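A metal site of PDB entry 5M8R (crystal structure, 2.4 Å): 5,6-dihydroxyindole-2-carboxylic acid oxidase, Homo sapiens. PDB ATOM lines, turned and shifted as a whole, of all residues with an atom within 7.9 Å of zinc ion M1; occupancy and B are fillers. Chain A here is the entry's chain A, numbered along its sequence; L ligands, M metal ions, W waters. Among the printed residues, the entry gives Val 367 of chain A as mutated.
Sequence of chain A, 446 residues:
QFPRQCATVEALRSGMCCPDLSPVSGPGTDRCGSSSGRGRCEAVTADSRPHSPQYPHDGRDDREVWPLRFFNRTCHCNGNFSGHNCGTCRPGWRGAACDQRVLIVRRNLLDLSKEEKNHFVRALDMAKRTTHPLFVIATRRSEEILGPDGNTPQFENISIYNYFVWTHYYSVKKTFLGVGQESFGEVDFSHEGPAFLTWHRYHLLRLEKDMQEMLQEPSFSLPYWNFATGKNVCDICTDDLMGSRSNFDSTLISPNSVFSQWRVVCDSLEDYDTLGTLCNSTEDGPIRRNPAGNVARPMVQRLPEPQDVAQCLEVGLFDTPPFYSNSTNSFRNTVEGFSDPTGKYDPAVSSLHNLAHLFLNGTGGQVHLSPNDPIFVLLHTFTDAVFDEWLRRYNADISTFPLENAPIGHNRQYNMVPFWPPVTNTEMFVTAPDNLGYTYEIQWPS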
ATOM      1  N   HIS A 168     -14.769 -22.384 -20.101  1.00  0.00           N
ATOM      2  CA  HIS A 168     -14.858 -21.825 -18.759  1.00  0.00           C
ATOM      3  C   HIS A 168     -15.955 -22.512 -17.948  1.00  0.00           C
ATOM      4  O   HIS A 168     -15.760 -22.807 -16.758  1.00  0.00           O
ATOM      5  CB  HIS A 168     -15.117 -20.306 -18.856  1.00  0.00           C
ATOM      6  CG  HIS A 168     -14.878 -19.543 -17.584  1.00  0.00           C
ATOM      7  ND1 HIS A 168     -15.895 -19.158 -16.737  1.00  0.00           N
ATOM      8  CD2 HIS A 168     -13.742 -19.030 -17.047  1.00  0.00           C
ATOM      9  CE1 HIS A 168     -15.392 -18.485 -15.713  1.00  0.00           C
ATOM     10  NE2 HIS A 168     -14.088 -18.384 -15.881  1.00  0.00           N
ATOM     11  N   SER A 171     -14.861 -25.999 -16.929  1.00  0.00           N
ATOM     12  CA  SER A 171     -13.845 -26.013 -15.873  1.00  0.00           C
ATOM     13  C   SER A 171     -14.425 -25.756 -14.489  1.00  0.00           C
ATOM     14  O   SER A 171     -13.822 -26.156 -13.497  1.00  0.00           O
ATOM     15  CB  SER A 171     -12.732 -24.980 -16.155  1.00  0.00           C
ATOM     16  OG  SER A 171     -13.153 -23.652 -15.793  1.00  0.00           O
ATOM     17  N   VAL A 172     -15.593 -25.099 -14.385  1.00  0.00           N
ATOM     18  CA  VAL A 172     -16.154 -24.786 -13.069  1.00  0.00           C
ATOM     19  C   VAL A 172     -17.373 -25.623 -12.721  1.00  0.00           C
ATOM     20  O   VAL A 172     -17.882 -25.480 -11.598  1.00  0.00           O
ATOM     21  CB  VAL A 172     -16.517 -23.301 -12.936  1.00  0.00           C
ATOM     22  CG1 VAL A 172     -15.319 -22.436 -13.242  1.00  0.00           C
ATOM     23  CG2 VAL A 172     -17.698 -22.963 -13.835  1.00  0.00           C
ATOM     24  N   ASP A 188     -13.243 -26.625  -8.551  1.00  0.00           N
ATOM     25  CA  ASP A 188     -13.180 -25.563  -9.552  1.00  0.00           C
ATOM     26  C   ASP A 188     -11.804 -25.615 -10.188  1.00  0.00           C
ATOM     27  O   ASP A 188     -10.806 -25.229  -9.574  1.00  0.00           O
ATOM     28  CB  ASP A 188     -13.473 -24.187  -8.913  1.00  0.00           C
ATOM     29  CG  ASP A 188     -13.684 -23.056  -9.953  1.00  0.00           C
ATOM     30  OD1 ASP A 188     -12.893 -22.923 -10.922  1.00  0.00           O
ATOM     31  OD2 ASP A 188     -14.639 -22.270  -9.771  1.00  0.00           O
ATOM     32  N   SER A 190     -10.378 -23.886 -12.435  1.00  0.00           N
ATOM     33  CA  SER A 190      -9.820 -22.647 -12.948  1.00  0.00           C
ATOM     34  C   SER A 190      -9.903 -21.461 -11.993  1.00  0.00           C
ATOM     35  O   SER A 190      -9.441 -20.381 -12.355  1.00  0.00           O
ATOM     36  CB  SER A 190     -10.517 -22.258 -14.252  1.00  0.00           C
ATOM     37  OG  SER A 190     -11.920 -22.178 -14.032  1.00  0.00           O
ATOM     38  N   HIS A 191     -10.456 -21.644 -10.789  1.00  0.00           N
ATOM     39  CA  HIS A 191     -10.553 -20.581  -9.798  1.00  0.00           C
ATOM     40  C   HIS A 191     -10.240 -21.150  -8.435  1.00  0.00           C
ATOM     41  O   HIS A 191     -10.172 -22.364  -8.249  1.00  0.00           O
ATOM     42  CB  HIS A 191     -11.951 -19.940  -9.768  1.00  0.00           C
ATOM     43  CG  HIS A 191     -12.444 -19.555 -11.111  1.00  0.00           C
ATOM     44  ND1 HIS A 191     -12.880 -20.470 -12.049  1.00  0.00           N
ATOM     45  CD2 HIS A 191     -12.520 -18.341 -11.711  1.00  0.00           C
ATOM     46  CE1 HIS A 191     -13.221 -19.836 -13.149  1.00  0.00           C
ATOM     47  NE2 HIS A 191     -13.026 -18.548 -12.974  1.00  0.00           N
ATOM     48  N   PHE A 196      -5.466 -20.323 -11.380  1.00  0.00           N
ATOM     49  CA  PHE A 196      -6.414 -19.295 -11.804  1.00  0.00           C
ATOM     50  C   PHE A 196      -5.820 -18.405 -12.903  1.00  0.00           C
ATOM     51  O   PHE A 196      -6.457 -18.157 -13.935  1.00  0.00           O
ATOM     52  CB  PHE A 196      -6.842 -18.448 -10.599  1.00  0.00           C
ATOM     53  CG  PHE A 196      -7.475 -17.126 -10.983  1.00  0.00           C
ATOM     54  CD1 PHE A 196      -8.773 -17.068 -11.467  1.00  0.00           C
ATOM     55  CD2 PHE A 196      -6.754 -15.938 -10.865  1.00  0.00           C
ATOM     56  CE1 PHE A 196      -9.340 -15.850 -11.841  1.00  0.00           C
ATOM     57  CE2 PHE A 196      -7.318 -14.732 -11.233  1.00  0.00           C
ATOM     58  CZ  PHE A 196      -8.608 -14.680 -11.714  1.00  0.00           C
ATOM     59  N   TRP A 199      -4.538 -20.555 -16.075  1.00  0.00           N
ATOM     60  CA  TRP A 199      -5.719 -21.022 -16.809  1.00  0.00           C
ATOM     61  C   TRP A 199      -6.294 -19.901 -17.667  1.00  0.00           C
ATOM     62  O   TRP A 199      -6.470 -20.059 -18.880  1.00  0.00           O
ATOM     63  CB  TRP A 199      -6.797 -21.561 -15.841  1.00  0.00           C
ATOM     64  CG  TRP A 199      -7.916 -22.323 -16.538  1.00  0.00           C
ATOM     65  CD1 TRP A 199      -8.053 -23.681 -16.607  1.00  0.00           C
ATOM     66  CD2 TRP A 199      -9.022 -21.766 -17.276  1.00  0.00           C
ATOM     67  NE1 TRP A 199      -9.169 -24.009 -17.352  1.00  0.00           N
ATOM     68  CE2 TRP A 199      -9.780 -22.858 -17.756  1.00  0.00           C
ATOM     69  CE3 TRP A 199      -9.434 -20.460 -17.580  1.00  0.00           C
ATOM     70  CZ2 TRP A 199     -10.959 -22.675 -18.534  1.00  0.00           C
ATOM     71  CZ3 TRP A 199     -10.611 -20.284 -18.342  1.00  0.00           C
ATOM     72  CH2 TRP A 199     -11.352 -21.386 -18.817  1.00  0.00           C
ATOM     73  N   HIS A 200      -6.614 -18.755 -17.048  1.00  0.00           N
ATOM     74  CA  HIS A 200      -7.271 -17.660 -17.774  1.00  0.00           C
ATOM     75  C   HIS A 200      -6.348 -17.051 -18.808  1.00  0.00           C
ATOM     76  O   HIS A 200      -6.834 -16.523 -19.808  1.00  0.00           O
ATOM     77  CB  HIS A 200      -7.787 -16.597 -16.800  1.00  0.00           C
ATOM     78  CG  HIS A 200      -9.034 -17.019 -16.075  1.00  0.00           C
ATOM     79  ND1 HIS A 200      -9.016 -17.874 -14.999  1.00  0.00           N
ATOM     80  CD2 HIS A 200     -10.347 -16.751 -16.321  1.00  0.00           C
ATOM     81  CE1 HIS A 200     -10.251 -18.099 -14.592  1.00  0.00           C
ATOM     82  NE2 HIS A 200     -11.077 -17.420 -15.364  1.00  0.00           N
ATOM     83  N   HIS A 203      -6.776 -19.345 -21.840  1.00  0.00           N
ATOM     84  CA  HIS A 203      -8.123 -19.007 -22.273  1.00  0.00           C
ATOM     85  C   HIS A 203      -8.123 -17.802 -23.215  1.00  0.00           C
ATOM     86  O   HIS A 203      -8.647 -17.869 -24.338  1.00  0.00           O
ATOM     87  CB  HIS A 203      -8.961 -18.722 -21.022  1.00  0.00           C
ATOM     88  CG  HIS A 203     -10.438 -18.742 -21.236  1.00  0.00           C
ATOM     89  ND1 HIS A 203     -11.295 -17.928 -20.522  1.00  0.00           N
ATOM     90  CD2 HIS A 203     -11.224 -19.508 -22.036  1.00  0.00           C
ATOM     91  CE1 HIS A 203     -12.538 -18.163 -20.901  1.00  0.00           C
ATOM     92  NE2 HIS A 203     -12.525 -19.123 -21.809  1.00  0.00           N
ATOM     93  N   GLU A 336      -6.690 -12.373  -7.729  1.00  0.00           N
ATOM     94  CA  GLU A 336      -7.957 -13.035  -7.982  1.00  0.00           C
ATOM     95  C   GLU A 336      -9.078 -12.349  -7.220  1.00  0.00           C
ATOM     96  O   GLU A 336     -10.185 -12.198  -7.741  1.00  0.00           O
ATOM     97  CB  GLU A 336      -7.893 -14.527  -7.628  1.00  0.00           C
ATOM     98  CG  GLU A 336      -9.226 -15.206  -7.973  1.00  0.00           C
ATOM     99  CD  GLU A 336      -9.243 -16.709  -7.816  1.00  0.00           C
ATOM    100  OE1 GLU A 336      -8.212 -17.288  -7.429  1.00  0.00           O
ATOM    101  OE2 GLU A 336     -10.314 -17.307  -8.101  1.00  0.00           O
ATOM    102  N   HIS A 353      -9.979  -8.574  -9.202  1.00  0.00           N
ATOM    103  CA  HIS A 353     -10.674  -9.307 -10.276  1.00  0.00           C
ATOM    104  C   HIS A 353     -12.068  -9.765  -9.858  1.00  0.00           C
ATOM    105  O   HIS A 353     -13.019  -9.664 -10.633  1.00  0.00           O
ATOM    106  CB  HIS A 353      -9.816 -10.498 -10.721  1.00  0.00           C
ATOM    107  CG  HIS A 353     -10.604 -11.659 -11.241  1.00  0.00           C
ATOM    108  ND1 HIS A 353     -11.026 -12.692 -10.436  1.00  0.00           N
ATOM    109  CD2 HIS A 353     -11.054 -11.943 -12.487  1.00  0.00           C
ATOM    110  CE1 HIS A 353     -11.700 -13.570 -11.155  1.00  0.00           C
ATOM    111  NE2 HIS A 353     -11.729 -13.140 -12.417  1.00  0.00           N
ATOM    112  N   ASN A 354     -12.210 -10.295  -8.636  1.00  0.00           N
ATOM    113  CA  ASN A 354     -13.536 -10.674  -8.161  1.00  0.00           C
ATOM    114  C   ASN A 354     -14.467  -9.460  -8.106  1.00  0.00           C
ATOM    115  O   ASN A 354     -15.634  -9.546  -8.514  1.00  0.00           O
ATOM    116  CB  ASN A 354     -13.439 -11.331  -6.786  1.00  0.00           C
ATOM    117  CG  ASN A 354     -12.945 -12.761  -6.841  1.00  0.00           C
ATOM    118  OD1 ASN A 354     -12.998 -13.421  -7.879  1.00  0.00           O
ATOM    119  ND2 ASN A 354     -12.502 -13.274  -5.709  1.00  0.00           N
ATOM    120  N   HIS A 357     -15.933  -8.352 -11.320  1.00  0.00           N
ATOM    121  CA  HIS A 357     -17.016  -9.234 -11.743  1.00  0.00           C
ATOM    122  C   HIS A 357     -18.315  -8.873 -11.055  1.00  0.00           C
ATOM    123  O   HIS A 357     -19.372  -8.778 -11.696  1.00  0.00           O
ATOM    124  CB  HIS A 357     -16.688 -10.688 -11.422  1.00  0.00           C
ATOM    125  CG  HIS A 357     -15.914 -11.409 -12.471  1.00  0.00           C
ATOM    126  ND1 HIS A 357     -16.492 -11.882 -13.640  1.00  0.00           N
ATOM    127  CD2 HIS A 357     -14.614 -11.791 -12.529  1.00  0.00           C
ATOM    128  CE1 HIS A 357     -15.576 -12.506 -14.360  1.00  0.00           C
ATOM    129  NE2 HIS A 357     -14.438 -12.463 -13.708  1.00  0.00           N
ATOM    130  N   GLN A 366     -21.516 -14.125 -12.459  1.00  0.00           N
ATOM    131  CA  GLN A 366     -21.749 -15.519 -12.125  1.00  0.00           C
ATOM    132  C   GLN A 366     -20.704 -16.379 -12.832  1.00  0.00           C
ATOM    133  O   GLN A 366     -20.602 -16.329 -14.058  1.00  0.00           O
ATOM    134  CB  GLN A 366     -23.149 -15.945 -12.539  1.00  0.00           C
ATOM    135  CG  GLN A 366     -24.219 -15.051 -11.999  1.00  0.00           C
ATOM    136  CD  GLN A 366     -25.587 -15.475 -12.509  1.00  0.00           C
ATOM    137  OE1 GLN A 366     -26.176 -14.797 -13.347  1.00  0.00           O
ATOM    138  NE2 GLN A 366     -26.071 -16.617 -12.041  1.00  0.00           N
ATOM    139  N   VAL A 367     -19.962 -17.170 -12.051  1.00  0.00           N
ATOM    140  CA  VAL A 367     -18.722 -17.776 -12.565  1.00  0.00           C
ATOM    141  C   VAL A 367     -19.001 -18.784 -13.686  1.00  0.00           C
ATOM    142  O   VAL A 367     -18.206 -18.901 -14.617  1.00  0.00           O
ATOM    143  CB  VAL A 367     -17.909 -18.380 -11.398  1.00  0.00           C
ATOM    144  CG1 VAL A 367     -18.567 -19.585 -10.843  1.00  0.00           C
ATOM    145  CG2 VAL A 367     -16.469 -18.700 -11.828  1.00  0.00           C
ATOM    146  N   HIS A 368     -20.140 -19.488 -13.645  1.00  0.00           N
ATOM    147  CA  HIS A 368     -20.449 -20.410 -14.733  1.00  0.00           C
ATOM    148  C   HIS A 368     -20.970 -19.715 -15.997  1.00  0.00           C
ATOM    149  O   HIS A 368     -21.161 -20.359 -17.027  1.00  0.00           O
ATOM    150  CB  HIS A 368     -21.488 -21.448 -14.267  1.00  0.00           C
ATOM    151  CG  HIS A 368     -22.893 -20.912 -14.304  1.00  0.00           C
ATOM    152  ND1 HIS A 368     -23.429 -20.137 -13.294  1.00  0.00           N
ATOM    153  CD2 HIS A 368     -23.858 -21.020 -15.259  1.00  0.00           C
ATOM    154  CE1 HIS A 368     -24.661 -19.797 -13.618  1.00  0.00           C
ATOM    155  NE2 HIS A 368     -24.947 -20.312 -14.797  1.00  0.00           N
ATOM    156  N   SER A 370     -20.037 -16.064 -16.722  1.00  0.00           N
ATOM    157  CA  SER A 370     -19.548 -14.709 -16.895  1.00  0.00           C
ATOM    158  C   SER A 370     -18.868 -14.435 -18.248  1.00  0.00           C
ATOM    159  O   SER A 370     -18.995 -13.296 -18.711  1.00  0.00           O
ATOM    160  CB  SER A 370     -18.654 -14.362 -15.704  1.00  0.00           C
ATOM    161  OG  SER A 370     -17.551 -15.238 -15.601  1.00  0.00           O
ATOM    162  N   PRO A 371     -18.239 -15.397 -18.950  1.00  0.00           N
ATOM    163  CA  PRO A 371     -17.726 -15.057 -20.299  1.00  0.00           C
ATOM    164  C   PRO A 371     -18.816 -14.674 -21.284  1.00  0.00           C
ATOM    165  O   PRO A 371     -18.480 -14.098 -22.333  1.00  0.00           O
ATOM    166  CB  PRO A 371     -17.016 -16.340 -20.766  1.00  0.00           C
ATOM    167  CG  PRO A 371     -16.757 -17.136 -19.526  1.00  0.00           C
ATOM    168  CD  PRO A 371     -17.881 -16.781 -18.589  1.00  0.00           C
ATOM    169  N   PHE A 376     -15.894  -9.706 -20.019  1.00  0.00           N
ATOM    170  CA  PHE A 376     -15.017 -10.723 -19.460  1.00  0.00           C
ATOM    171  C   PHE A 376     -13.634 -10.701 -20.127  1.00  0.00           C
ATOM    172  O   PHE A 376     -12.602 -10.734 -19.439  1.00  0.00           O
ATOM    173  CB  PHE A 376     -15.698 -12.087 -19.630  1.00  0.00           C
ATOM    174  CG  PHE A 376     -14.901 -13.260 -19.084  1.00  0.00           C
ATOM    175  CD1 PHE A 376     -13.881 -13.821 -19.820  1.00  0.00           C
ATOM    176  CD2 PHE A 376     -15.212 -13.801 -17.848  1.00  0.00           C
ATOM    177  CE1 PHE A 376     -13.163 -14.903 -19.345  1.00  0.00           C
ATOM    178  CE2 PHE A 376     -14.508 -14.879 -17.363  1.00  0.00           C
ATOM    179  CZ  PHE A 376     -13.468 -15.437 -18.114  1.00  0.00           C
ATOM    180  N   LEU A 379     -11.793  -7.555 -18.963  1.00  0.00           N
ATOM    181  CA  LEU A 379     -11.525  -7.714 -17.542  1.00  0.00           C
ATOM    182  C   LEU A 379     -10.368  -8.688 -17.294  1.00  0.00           C
ATOM    183  O   LEU A 379      -9.546  -8.482 -16.388  1.00  0.00           O
ATOM    184  CB  LEU A 379     -12.818  -8.190 -16.853  1.00  0.00           C
ATOM    185  CG  LEU A 379     -12.976  -8.368 -15.347  1.00  0.00           C
ATOM    186  CD1 LEU A 379     -14.461  -8.611 -15.069  1.00  0.00           C
ATOM    187  CD2 LEU A 379     -12.166  -9.549 -14.820  1.00  0.00           C
ATOM    188  N   HIS A 380     -10.278  -9.749 -18.102  1.00  0.00           N
ATOM    189  CA  HIS A 380      -9.201 -10.727 -17.918  1.00  0.00           C
ATOM    190  C   HIS A 380      -7.913 -10.408 -18.667  1.00  0.00           C
ATOM    191  O   HIS A 380      -6.850 -10.794 -18.196  1.00  0.00           O
ATOM    192  CB  HIS A 380      -9.672 -12.132 -18.303  1.00  0.00           C
ATOM    193  CG  HIS A 380     -10.165 -12.896 -17.118  1.00  0.00           C
ATOM    194  ND1 HIS A 380      -9.319 -13.413 -16.163  1.00  0.00           N
ATOM    195  CD2 HIS A 380     -11.424 -13.123 -16.675  1.00  0.00           C
ATOM    196  CE1 HIS A 380     -10.031 -13.951 -15.199  1.00  0.00           C
ATOM    197  NE2 HIS A 380     -11.310 -13.808 -15.491  1.00  0.00           N
HETATM  198  O1  LIG L   1     -14.016 -15.491 -11.587  1.00  0.00           O
HETATM  199  C1  LIG L   1     -16.588 -14.219  -5.572  1.00  0.00           C
HETATM  200  O2  LIG L   1     -16.207 -13.056  -5.266  1.00  0.00           O
HETATM  201  O3  LIG L   1     -17.219 -14.925  -4.736  1.00  0.00           O
HETATM  202  N1  LIG L   1     -16.970 -16.081  -7.127  1.00  0.00           N
HETATM  203  C2  LIG L   1     -16.300 -14.794  -6.960  1.00  0.00           C
HETATM  204  C3  LIG L   1     -16.827 -13.785  -7.964  1.00  0.00           C
HETATM  205  N2  LIG L   1     -16.668 -14.204  -9.331  1.00  0.00           N
HETATM  206  C4  LIG L   1     -15.350 -14.673  -9.822  1.00  0.00           C
HETATM  207  C5  LIG L   1     -17.840 -14.143 -10.258  1.00  0.00           C
HETATM  208  C6  LIG L   1     -15.234 -15.051 -11.084  1.00  0.00           C
HETATM  209  C7  LIG L   1     -17.719 -14.514 -11.524  1.00  0.00           C
HETATM  210  C8  LIG L   1     -16.388 -14.991 -12.034  1.00  0.00           C
HETATM  211  O4  LIG L   1     -16.226 -15.326 -13.161  1.00  0.00           O
HETATM  212 ZN    ZN M   1     -12.935 -17.330 -14.626  1.00  0.00          ZN
HETATM  213 ZN    ZN M   2     -12.868 -13.830 -14.014  1.00  0.00          ZN
HETATM  214  O   HOH W   1     -13.876 -15.561 -14.055  1.00  0.00           O
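A ring nitrogen (NE2) of His 191 lies close to an oxygen (O1) of the ligand.
An oxygen (O1) of the ligand lies close to a ring nitrogen (NE2) of His 353 (3.4 Å).
OG of Ser 370 is in hydrogen-bond range of O4 of the ligand.
A ring nitrogen (ND1) of His 357 sits close to an oxygen (O4) of the ligand, 3.5 Å away.
O of Phe 196 lies within hydrogen-bond range of ND1 of His 200 (2.8 Å).
A ring nitrogen (ND1) of His 168 lies close to the backbone carbonyl oxygen of Val 367, at 3.1 Å.
OG of Ser 171 sits at hydrogen-bond distance from O of His 168 (2.9 Å).
A ring nitrogen (ND1) of His 191 is in hydrogen-bond range of the side-chain hydroxyl (OG) of Ser 190, at 2.8 Å.
The side-chain carboxylate of Asp 188 sits at hydrogen-bond distance from a ring nitrogen (ND1) of His 191, at 2.7 Å.
Phe 376 touches zinc ion M1.
NE2 of His 380 touches zinc ion M1, 3.97 Å away.
Within 4 Å of zinc ion M1: His 168, His 191, His 200, Phe 376 and His 380.
Zinc ion M1 is bound by NE2 of His 200 (2.0 Å), NE2 of His 168 (2.0 Å), NE2 of His 191 (2.1 Å) and water W1 (2.1 Å).
Zinc ion M1 has four donor atoms within binding distance.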
